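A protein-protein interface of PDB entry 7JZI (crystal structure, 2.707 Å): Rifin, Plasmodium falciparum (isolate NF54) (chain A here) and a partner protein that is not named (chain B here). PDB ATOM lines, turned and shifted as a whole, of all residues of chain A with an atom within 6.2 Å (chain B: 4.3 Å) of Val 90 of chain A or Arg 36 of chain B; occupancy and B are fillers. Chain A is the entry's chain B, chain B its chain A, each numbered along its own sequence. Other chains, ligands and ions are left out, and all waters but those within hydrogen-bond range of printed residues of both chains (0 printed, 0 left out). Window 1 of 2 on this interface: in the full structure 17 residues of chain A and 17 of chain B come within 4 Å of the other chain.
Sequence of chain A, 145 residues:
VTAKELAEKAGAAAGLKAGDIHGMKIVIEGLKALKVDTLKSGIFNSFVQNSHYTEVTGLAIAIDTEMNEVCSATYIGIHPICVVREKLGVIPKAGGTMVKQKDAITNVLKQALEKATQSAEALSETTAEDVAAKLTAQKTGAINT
The backbone carbonyl oxygen (O) of Val 90 of chain A is in hydrogen-bond range of the guanidinium group (NH1) of Arg 36 of chain B (3.3 Å).
The side-chain hydroxyl (OH) of Tyr 45 of chain B sits at hydrogen-bond distance from the guanidinium group (NE) of Arg 85 of chain A, 3.3 Å away.
Of the 14 printed residues of chain A, 5 touch a printed residue of chain B.
Printed residues of chain A that touch a printed residue of chain B: Arg 85, Val 90, Pro 92, Met 98 and Gln 101.
Among the printed residues, merely in contact across the chains: Val 90 of chain A with Tyr 45 of chain B (3.3 Å), Pro 92 of chain A with Arg 36 of chain B (3.4 Å), Pro 92 of chain A with Ile 79 of chain B (3.7 Å), Pro 92 of chain A with Trp 86 of chain B (3.4 Å), Met 98 of chain A with Trp 86 of chain B (3.3 Å) and Gln 101 of chain A with Tyr 45 of chain B (3.6 Å).
Printed residues of chain B within 4 Å of Pro 92 of chain A: Arg 36 (3.4 Å), Ile 79 (3.7 Å) and Trp 86 (3.4 Å).
Printed residues of chain B within 4 Å of Met 98 of chain A: Trp 86 (3.3 Å).
Arg 36 of chain B touches just these residues of chain A: Val 90 and Pro 92.
Printed residues of chain A within 4 Å of Tyr 45 of chain B: Arg 85, Val 90 and Gln 101.
The nearest residue of chain A that does not touch Arg 36 of chain B is Ile 91 of chain A (4.6 Å).
The side-chain carboxylate (OD1) of Asp 47 of chain B is in salt-bridge range of the guanidinium group (NE) of Arg 36 of chain B, 2.7 Å away.
The backbone NH of Arg 36 of chain B sits at hydrogen-bond distance from the backbone carbonyl oxygen of Ile 79 of chain B.
The side-chain amide nitrogen (NE2) of Gln 101 of chain A lies close to the guanidinium group (NE) of Arg 85 of chain A, 3.1 Å away.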
ATOM      1  N   ARG A  85      -8.696   0.270  -7.791  1.00  0.00           N
ATOM      2  CA  ARG A  85      -7.914   1.509  -7.990  1.00  0.00           C
ATOM      3  C   ARG A  85      -6.907   1.654  -6.851  1.00  0.00           C
ATOM      4  O   ARG A  85      -5.791   2.111  -7.114  1.00  0.00           O
ATOM      5  CB  ARG A  85      -8.852   2.713  -8.036  1.00  0.00           C
ATOM      6  CG  ARG A  85      -9.292   3.121  -9.432  1.00  0.00           C
ATOM      7  CD  ARG A  85     -10.292   4.256  -9.354  1.00  0.00           C
ATOM      8  NE  ARG A  85     -10.480   4.904 -10.640  1.00  0.00           N
ATOM      9  CZ  ARG A  85     -11.393   5.832 -10.883  1.00  0.00           C
ATOM     10  NH1 ARG A  85     -11.486   6.370 -12.084  1.00  0.00           N
ATOM     11  NH2 ARG A  85     -12.211   6.219  -9.925  1.00  0.00           N
ATOM     12  N   GLU A  86      -7.281   1.279  -5.631  1.00  0.00           N
ATOM     13  CA  GLU A  86      -6.374   1.496  -4.477  1.00  0.00           C
ATOM     14  C   GLU A  86      -5.080   0.731  -4.722  1.00  0.00           C
ATOM     15  O   GLU A  86      -4.009   1.269  -4.416  1.00  0.00           O
ATOM     16  CB  GLU A  86      -7.017   0.985  -3.193  1.00  0.00           C
ATOM     17  CG  GLU A  86      -8.231   1.781  -2.759  1.00  0.00           C
ATOM     18  CD  GLU A  86      -8.953   1.195  -1.558  1.00  0.00           C
ATOM     19  OE1 GLU A  86      -8.760  -0.004  -1.281  1.00  0.00           O
ATOM     20  OE2 GLU A  86      -9.701   1.942  -0.899  1.00  0.00           O
ATOM     21  N   LYS A  87      -5.190  -0.482  -5.247  1.00  0.00           N
ATOM     22  CA  LYS A  87      -3.994  -1.298  -5.554  1.00  0.00           C
ATOM     23  C   LYS A  87      -3.182  -0.600  -6.639  1.00  0.00           C
ATOM     24  O   LYS A  87      -1.953  -0.664  -6.581  1.00  0.00           O
ATOM     25  CB  LYS A  87      -4.448  -2.703  -5.947  1.00  0.00           C
ATOM     26  CG  LYS A  87      -5.573  -3.254  -5.080  1.00  0.00           C
ATOM     27  CD  LYS A  87      -5.939  -4.691  -5.373  1.00  0.00           C
ATOM     28  CE  LYS A  87      -7.049  -5.198  -4.477  1.00  0.00           C
ATOM     29  NZ  LYS A  87      -7.301  -6.646  -4.670  1.00  0.00           N
ATOM     30  N   LEU A  88      -3.858   0.021  -7.601  1.00  0.00           N
ATOM     31  CA  LEU A  88      -3.161   0.694  -8.722  1.00  0.00           C
ATOM     32  C   LEU A  88      -2.325   1.850  -8.183  1.00  0.00           C
ATOM     33  O   LEU A  88      -1.301   2.162  -8.793  1.00  0.00           O
ATOM     34  CB  LEU A  88      -4.186   1.168  -9.752  1.00  0.00           C
ATOM     35  CG  LEU A  88      -4.874   0.073 -10.564  1.00  0.00           C
ATOM     36  CD1 LEU A  88      -6.022   0.652 -11.374  1.00  0.00           C
ATOM     37  CD2 LEU A  88      -3.883  -0.626 -11.479  1.00  0.00           C
ATOM     38  N   GLY A  89      -2.754   2.462  -7.084  1.00  0.00           N
ATOM     39  CA  GLY A  89      -1.952   3.535  -6.475  1.00  0.00           C
ATOM     40  C   GLY A  89      -2.422   4.902  -6.901  1.00  0.00           C
ATOM     41  O   GLY A  89      -1.751   5.878  -6.570  1.00  0.00           O
ATOM     42  N   VAL A  90      -3.566   4.969  -7.567  1.00  0.00           N
ATOM     43  CA  VAL A  90      -4.087   6.256  -8.095  1.00  0.00           C
ATOM     44  C   VAL A  90      -4.832   7.000  -6.995  1.00  0.00           C
ATOM     45  O   VAL A  90      -5.313   8.099  -7.274  1.00  0.00           O
ATOM     46  CB  VAL A  90      -4.979   6.012  -9.320  1.00  0.00           C
ATOM     47  CG1 VAL A  90      -4.178   5.429 -10.470  1.00  0.00           C
ATOM     48  CG2 VAL A  90      -6.147   5.106  -8.982  1.00  0.00           C
ATOM     49  N   ILE A  91      -4.933   6.428  -5.802  1.00  0.00           N
ATOM     50  CA  ILE A  91      -5.552   7.197  -4.687  1.00  0.00           C
ATOM     51  C   ILE A  91      -4.421   8.025  -4.065  1.00  0.00           C
ATOM     52  O   ILE A  91      -3.426   7.420  -3.649  1.00  0.00           O
ATOM     53  CB  ILE A  91      -6.327   6.316  -3.695  1.00  0.00           C
ATOM     54  CG1 ILE A  91      -7.754   6.048  -4.176  1.00  0.00           C
ATOM     55  CG2 ILE A  91      -6.338   6.945  -2.312  1.00  0.00           C
ATOM     56  CD1 ILE A  91      -7.851   5.098  -5.342  1.00  0.00           C
ATOM     57  N   PRO A  92      -4.488   9.376  -4.014  1.00  0.00           N
ATOM     58  CA  PRO A  92      -3.344  10.190  -3.599  1.00  0.00           C
ATOM     59  C   PRO A  92      -3.352  10.583  -2.135  1.00  0.00           C
ATOM     60  O   PRO A  92      -4.355  11.067  -1.599  1.00  0.00           O
ATOM     61  CB  PRO A  92      -3.473  11.417  -4.501  1.00  0.00           C
ATOM     62  CG  PRO A  92      -4.968  11.569  -4.681  1.00  0.00           C
ATOM     63  CD  PRO A  92      -5.595  10.199  -4.529  1.00  0.00           C
ATOM     64  N   MET A  98       1.100  12.948  -8.910  1.00  0.00           N
ATOM     65  CA  MET A  98       0.009  12.328  -9.644  1.00  0.00           C
ATOM     66  C   MET A  98       0.520  11.057 -10.298  1.00  0.00           C
ATOM     67  O   MET A  98       1.677  10.979 -10.725  1.00  0.00           O
ATOM     68  CB  MET A  98      -0.592  13.237 -10.718  1.00  0.00           C
ATOM     69  CG  MET A  98      -2.098  12.986 -10.805  1.00  0.00           C
ATOM     70  SD  MET A  98      -3.102  13.534 -12.218  1.00  0.00           S
ATOM     71  CE  MET A  98      -2.725  15.271 -12.392  1.00  0.00           C
ATOM     72  N   VAL A  99      -0.351  10.060 -10.374  1.00  0.00           N
ATOM     73  CA  VAL A  99      -0.034   8.794 -11.012  1.00  0.00           C
ATOM     74  C   VAL A  99      -1.189   8.461 -11.940  1.00  0.00           C
ATOM     75  O   VAL A  99      -2.326   8.305 -11.483  1.00  0.00           O
ATOM     76  CB  VAL A  99       0.213   7.675  -9.986  1.00  0.00           C
ATOM     77  CG1 VAL A  99      -0.868   7.664  -8.924  1.00  0.00           C
ATOM     78  CG2 VAL A  99       0.288   6.325 -10.697  1.00  0.00           C
ATOM     79  N   LYS A 100      -0.917   8.394 -13.240  1.00  0.00           N
ATOM     80  CA  LYS A 100      -1.998   8.226 -14.198  1.00  0.00           C
ATOM     81  C   LYS A 100      -2.528   6.799 -14.178  1.00  0.00           C
ATOM     82  O   LYS A 100      -1.764   5.833 -14.089  1.00  0.00           O
ATOM     83  CB  LYS A 100      -1.527   8.574 -15.612  1.00  0.00           C
ATOM     84  CG  LYS A 100      -1.032  10.007 -15.798  1.00  0.00           C
ATOM     85  CD  LYS A 100      -2.211  10.976 -15.724  1.00  0.00           C
ATOM     86  CE  LYS A 100      -1.828  12.347 -15.189  1.00  0.00           C
ATOM     87  NZ  LYS A 100      -3.032  13.223 -15.132  1.00  0.00           N
ATOM     88  N   GLN A 101      -3.847   6.655 -14.224  1.00  0.00           N
ATOM     89  CA  GLN A 101      -4.445   5.303 -14.137  1.00  0.00           C
ATOM     90  C   GLN A 101      -3.961   4.469 -15.319  1.00  0.00           C
ATOM     91  O   GLN A 101      -3.508   3.345 -15.092  1.00  0.00           O
ATOM     92  CB  GLN A 101      -5.965   5.420 -14.078  1.00  0.00           C
ATOM     93  CG  GLN A 101      -6.702   4.097 -13.993  1.00  0.00           C
ATOM     94  CD  GLN A 101      -8.174   4.370 -13.837  1.00  0.00           C
ATOM     95  OE1 GLN A 101      -9.013   3.760 -14.491  1.00  0.00           O
ATOM     96  NE2 GLN A 101      -8.497   5.328 -12.988  1.00  0.00           N
ATOM     97  N   LYS A 102      -4.049   5.009 -16.532  1.00  0.00           N
ATOM     98  CA  LYS A 102      -3.674   4.210 -17.689  1.00  0.00           C
ATOM     99  C   LYS A 102      -2.243   3.711 -17.565  1.00  0.00           C
ATOM    100  O   LYS A 102      -1.944   2.578 -17.956  1.00  0.00           O
ATOM    101  CB  LYS A 102      -3.872   5.034 -18.966  1.00  0.00           C
ATOM    102  CG  LYS A 102      -3.375   4.425 -20.279  1.00  0.00           C
ATOM    103  CD  LYS A 102      -1.968   4.876 -20.634  1.00  0.00           C
ATOM    104  CE  LYS A 102      -1.581   4.393 -22.019  1.00  0.00           C
ATOM    105  NZ  LYS A 102      -0.988   3.033 -22.000  1.00  0.00           N
ATOM    106  N   ALA A 104      -0.665   3.016 -14.716  1.00  0.00           N
ATOM    107  CA  ALA A 104      -0.672   1.934 -13.735  1.00  0.00           C
ATOM    108  C   ALA A 104      -1.245   0.653 -14.328  1.00  0.00           C
ATOM    109  O   ALA A 104      -0.727  -0.443 -14.076  1.00  0.00           O
ATOM    110  CB  ALA A 104      -1.466   2.354 -12.500  1.00  0.00           C
ATOM    111  N   PHE B  35      -8.679  19.232 -10.937  1.00  0.00           N
ATOM    112  CA  PHE B  35      -9.603  19.155  -9.816  1.00  0.00           C
ATOM    113  C   PHE B  35     -10.243  17.772  -9.799  1.00  0.00           C
ATOM    114  O   PHE B  35     -10.539  17.204 -10.854  1.00  0.00           O
ATOM    115  CB  PHE B  35     -10.686  20.230  -9.907  1.00  0.00           C
ATOM    116  CG  PHE B  35     -10.480  21.380  -8.971  1.00  0.00           C
ATOM    117  CD1 PHE B  35     -10.512  21.191  -7.605  1.00  0.00           C
ATOM    118  CD2 PHE B  35     -10.289  22.662  -9.462  1.00  0.00           C
ATOM    119  CE1 PHE B  35     -10.324  22.253  -6.742  1.00  0.00           C
ATOM    120  CE2 PHE B  35     -10.111  23.725  -8.609  1.00  0.00           C
ATOM    121  CZ  PHE B  35     -10.125  23.523  -7.247  1.00  0.00           C
ATOM    122  N   ARG B  36     -10.484  17.243  -8.599  1.00  0.00           N
ATOM    123  CA  ARG B  36     -11.028  15.902  -8.422  1.00  0.00           C
ATOM    124  C   ARG B  36     -12.142  15.943  -7.390  1.00  0.00           C
ATOM    125  O   ARG B  36     -11.923  16.357  -6.244  1.00  0.00           O
ATOM    126  CB  ARG B  36      -9.950  14.907  -7.992  1.00  0.00           C
ATOM    127  CG  ARG B  36     -10.508  13.556  -7.578  1.00  0.00           C
ATOM    128  CD  ARG B  36      -9.420  12.549  -7.258  1.00  0.00           C
ATOM    129  NE  ARG B  36      -8.608  12.174  -8.412  1.00  0.00           N
ATOM    130  CZ  ARG B  36      -7.721  11.182  -8.385  1.00  0.00           C
ATOM    131  NH1 ARG B  36      -7.551  10.484  -7.271  1.00  0.00           N
ATOM    132  NH2 ARG B  36      -7.009  10.878  -9.462  1.00  0.00           N
ATOM    133  N   LEU B  37     -13.331  15.524  -7.815  1.00  0.00           N
ATOM    134  CA  LEU B  37     -14.489  15.359  -6.947  1.00  0.00           C
ATOM    135  C   LEU B  37     -14.562  13.913  -6.463  1.00  0.00           C
ATOM    136  O   LEU B  37     -14.489  12.981  -7.267  1.00  0.00           O
ATOM    137  CB  LEU B  37     -15.764  15.746  -7.696  1.00  0.00           C
ATOM    138  CG  LEU B  37     -17.061  15.691  -6.894  1.00  0.00           C
ATOM    139  CD1 LEU B  37     -17.056  16.709  -5.784  1.00  0.00           C
ATOM    140  CD2 LEU B  37     -18.256  15.883  -7.816  1.00  0.00           C
ATOM    141  N   GLU B  38     -14.713  13.732  -5.154  1.00  0.00           N
ATOM    142  CA  GLU B  38     -14.616  12.442  -4.493  1.00  0.00           C
ATOM    143  C   GLU B  38     -15.850  12.213  -3.636  1.00  0.00           C
ATOM    144  O   GLU B  38     -16.373  13.154  -3.037  1.00  0.00           O
ATOM    145  CB  GLU B  38     -13.381  12.386  -3.582  1.00  0.00           C
ATOM    146  CG  GLU B  38     -12.184  11.630  -4.120  1.00  0.00           C
ATOM    147  CD  GLU B  38     -11.147  11.379  -3.039  1.00  0.00           C
ATOM    148  OE1 GLU B  38     -10.052  10.867  -3.366  1.00  0.00           O
ATOM    149  OE2 GLU B  38     -11.430  11.701  -1.862  1.00  0.00           O
ATOM    150  N   TYR B  45     -14.265   8.711  -8.082  1.00  0.00           N
ATOM    151  CA  TYR B  45     -13.898  10.132  -8.299  1.00  0.00           C
ATOM    152  C   TYR B  45     -14.014  10.613  -9.749  1.00  0.00           C
ATOM    153  O   TYR B  45     -13.997   9.771 -10.653  1.00  0.00           O
ATOM    154  CB  TYR B  45     -12.478  10.369  -7.778  1.00  0.00           C
ATOM    155  CG  TYR B  45     -11.371   9.551  -8.391  1.00  0.00           C
ATOM    156  CD1 TYR B  45     -10.753   8.541  -7.675  1.00  0.00           C
ATOM    157  CD2 TYR B  45     -10.903   9.821  -9.664  1.00  0.00           C
ATOM    158  CE1 TYR B  45      -9.721   7.799  -8.222  1.00  0.00           C
ATOM    159  CE2 TYR B  45      -9.879   9.084 -10.229  1.00  0.00           C
ATOM    160  CZ  TYR B  45      -9.282   8.073  -9.502  1.00  0.00           C
ATOM    161  OH  TYR B  45      -8.272   7.352 -10.060  1.00  0.00           O
ATOM    162  N   SER B  46     -14.115  11.930  -9.960  1.00  0.00           N
ATOM    163  CA  SER B  46     -14.066  12.501 -11.300  1.00  0.00           C
ATOM    164  C   SER B  46     -12.969  13.548 -11.345  1.00  0.00           C
ATOM    165  O   SER B  46     -12.895  14.415 -10.464  1.00  0.00           O
ATOM    166  CB  SER B  46     -15.398  13.140 -11.711  1.00  0.00           C
ATOM    167  OG  SER B  46     -16.455  12.204 -11.689  1.00  0.00           O
ATOM    168  N   ASP B  47     -12.121  13.453 -12.365  1.00  0.00           N
ATOM    169  CA  ASP B  47     -11.069  14.420 -12.631  1.00  0.00           C
ATOM    170  C   ASP B  47     -11.501  15.348 -13.758  1.00  0.00           C
ATOM    171  O   ASP B  47     -12.137  14.914 -14.724  1.00  0.00           O
ATOM    172  CB  ASP B  47      -9.769  13.712 -13.023  1.00  0.00           C
ATOM    173  CG  ASP B  47      -9.021  13.130 -11.829  1.00  0.00           C
ATOM    174  OD1 ASP B  47      -9.456  13.342 -10.673  1.00  0.00           O
ATOM    175  OD2 ASP B  47      -7.987  12.450 -12.049  1.00  0.00           O
ATOM    176  N   ARG B  77     -16.351  15.674  -1.668  1.00  0.00           N
ATOM    177  CA  ARG B  77     -15.267  16.575  -1.286  1.00  0.00           C
ATOM    178  C   ARG B  77     -14.256  16.671  -2.424  1.00  0.00           C
ATOM    179  O   ARG B  77     -14.194  15.804  -3.293  1.00  0.00           O
ATOM    180  CB  ARG B  77     -14.588  16.101  -0.002  1.00  0.00           C
ATOM    181  CG  ARG B  77     -13.647  14.932  -0.233  1.00  0.00           C
ATOM    182  CD  ARG B  77     -12.969  14.453   1.043  1.00  0.00           C
ATOM    183  NE  ARG B  77     -12.079  13.323   0.776  1.00  0.00           N
ATOM    184  CZ  ARG B  77     -11.381  12.676   1.707  1.00  0.00           C
ATOM    185  NH1 ARG B  77     -11.472  13.035   2.979  1.00  0.00           N
ATOM    186  NH2 ARG B  77     -10.588  11.665   1.364  1.00  0.00           N
ATOM    187  N   CYS B  78     -13.449  17.723  -2.410  1.00  0.00           N
ATOM    188  CA  CYS B  78     -12.547  17.988  -3.517  1.00  0.00           C
ATOM    189  C   CYS B  78     -11.087  17.829  -3.112  1.00  0.00           C
ATOM    190  O   CYS B  78     -10.712  17.919  -1.939  1.00  0.00           O
ATOM    191  CB  CYS B  78     -12.780  19.400  -4.069  1.00  0.00           C
ATOM    192  SG  CYS B  78     -14.512  19.849  -4.512  1.00  0.00           S
ATOM    193  N   ILE B  79     -10.263  17.608  -4.129  1.00  0.00           N
ATOM    194  CA  ILE B  79      -8.819  17.748  -4.022  1.00  0.00           C
ATOM    195  C   ILE B  79      -8.356  18.337  -5.341  1.00  0.00           C
ATOM    196  O   ILE B  79      -9.028  18.217  -6.366  1.00  0.00           O
ATOM    197  CB  ILE B  79      -8.054  16.431  -3.741  1.00  0.00           C
ATOM    198  CG1 ILE B  79      -8.357  15.370  -4.797  1.00  0.00           C
ATOM    199  CG2 ILE B  79      -8.377  15.899  -2.436  1.00  0.00           C
ATOM    200  CD1 ILE B  79      -7.738  14.031  -4.509  1.00  0.00           C
ATOM    201  N   TRP B  86      -0.223  16.875  -4.883  1.00  0.00           N
ATOM    202  CA  TRP B  86      -1.684  16.873  -4.658  1.00  0.00           C
ATOM    203  C   TRP B  86      -1.941  17.695  -3.408  1.00  0.00           C
ATOM    204  O   TRP B  86      -1.059  17.763  -2.556  1.00  0.00           O
ATOM    205  CB  TRP B  86      -2.233  15.456  -4.501  1.00  0.00           C
ATOM    206  CG  TRP B  86      -2.588  14.740  -5.764  1.00  0.00           C
ATOM    207  CD1 TRP B  86      -1.852  13.786  -6.400  1.00  0.00           C
ATOM    208  CD2 TRP B  86      -3.798  14.885  -6.521  1.00  0.00           C
ATOM    209  NE1 TRP B  86      -2.516  13.338  -7.508  1.00  0.00           N
ATOM    210  CE2 TRP B  86      -3.711  13.998  -7.611  1.00  0.00           C
ATOM    211  CE3 TRP B  86      -4.937  15.683  -6.392  1.00  0.00           C
ATOM    212  CZ2 TRP B  86      -4.720  13.889  -8.564  1.00  0.00           C
ATOM    213  CZ3 TRP B  86      -5.932  15.578  -7.337  1.00  0.00           C
ATOM    214  CH2 TRP B  86      -5.824  14.691  -8.405  1.00  0.00           C
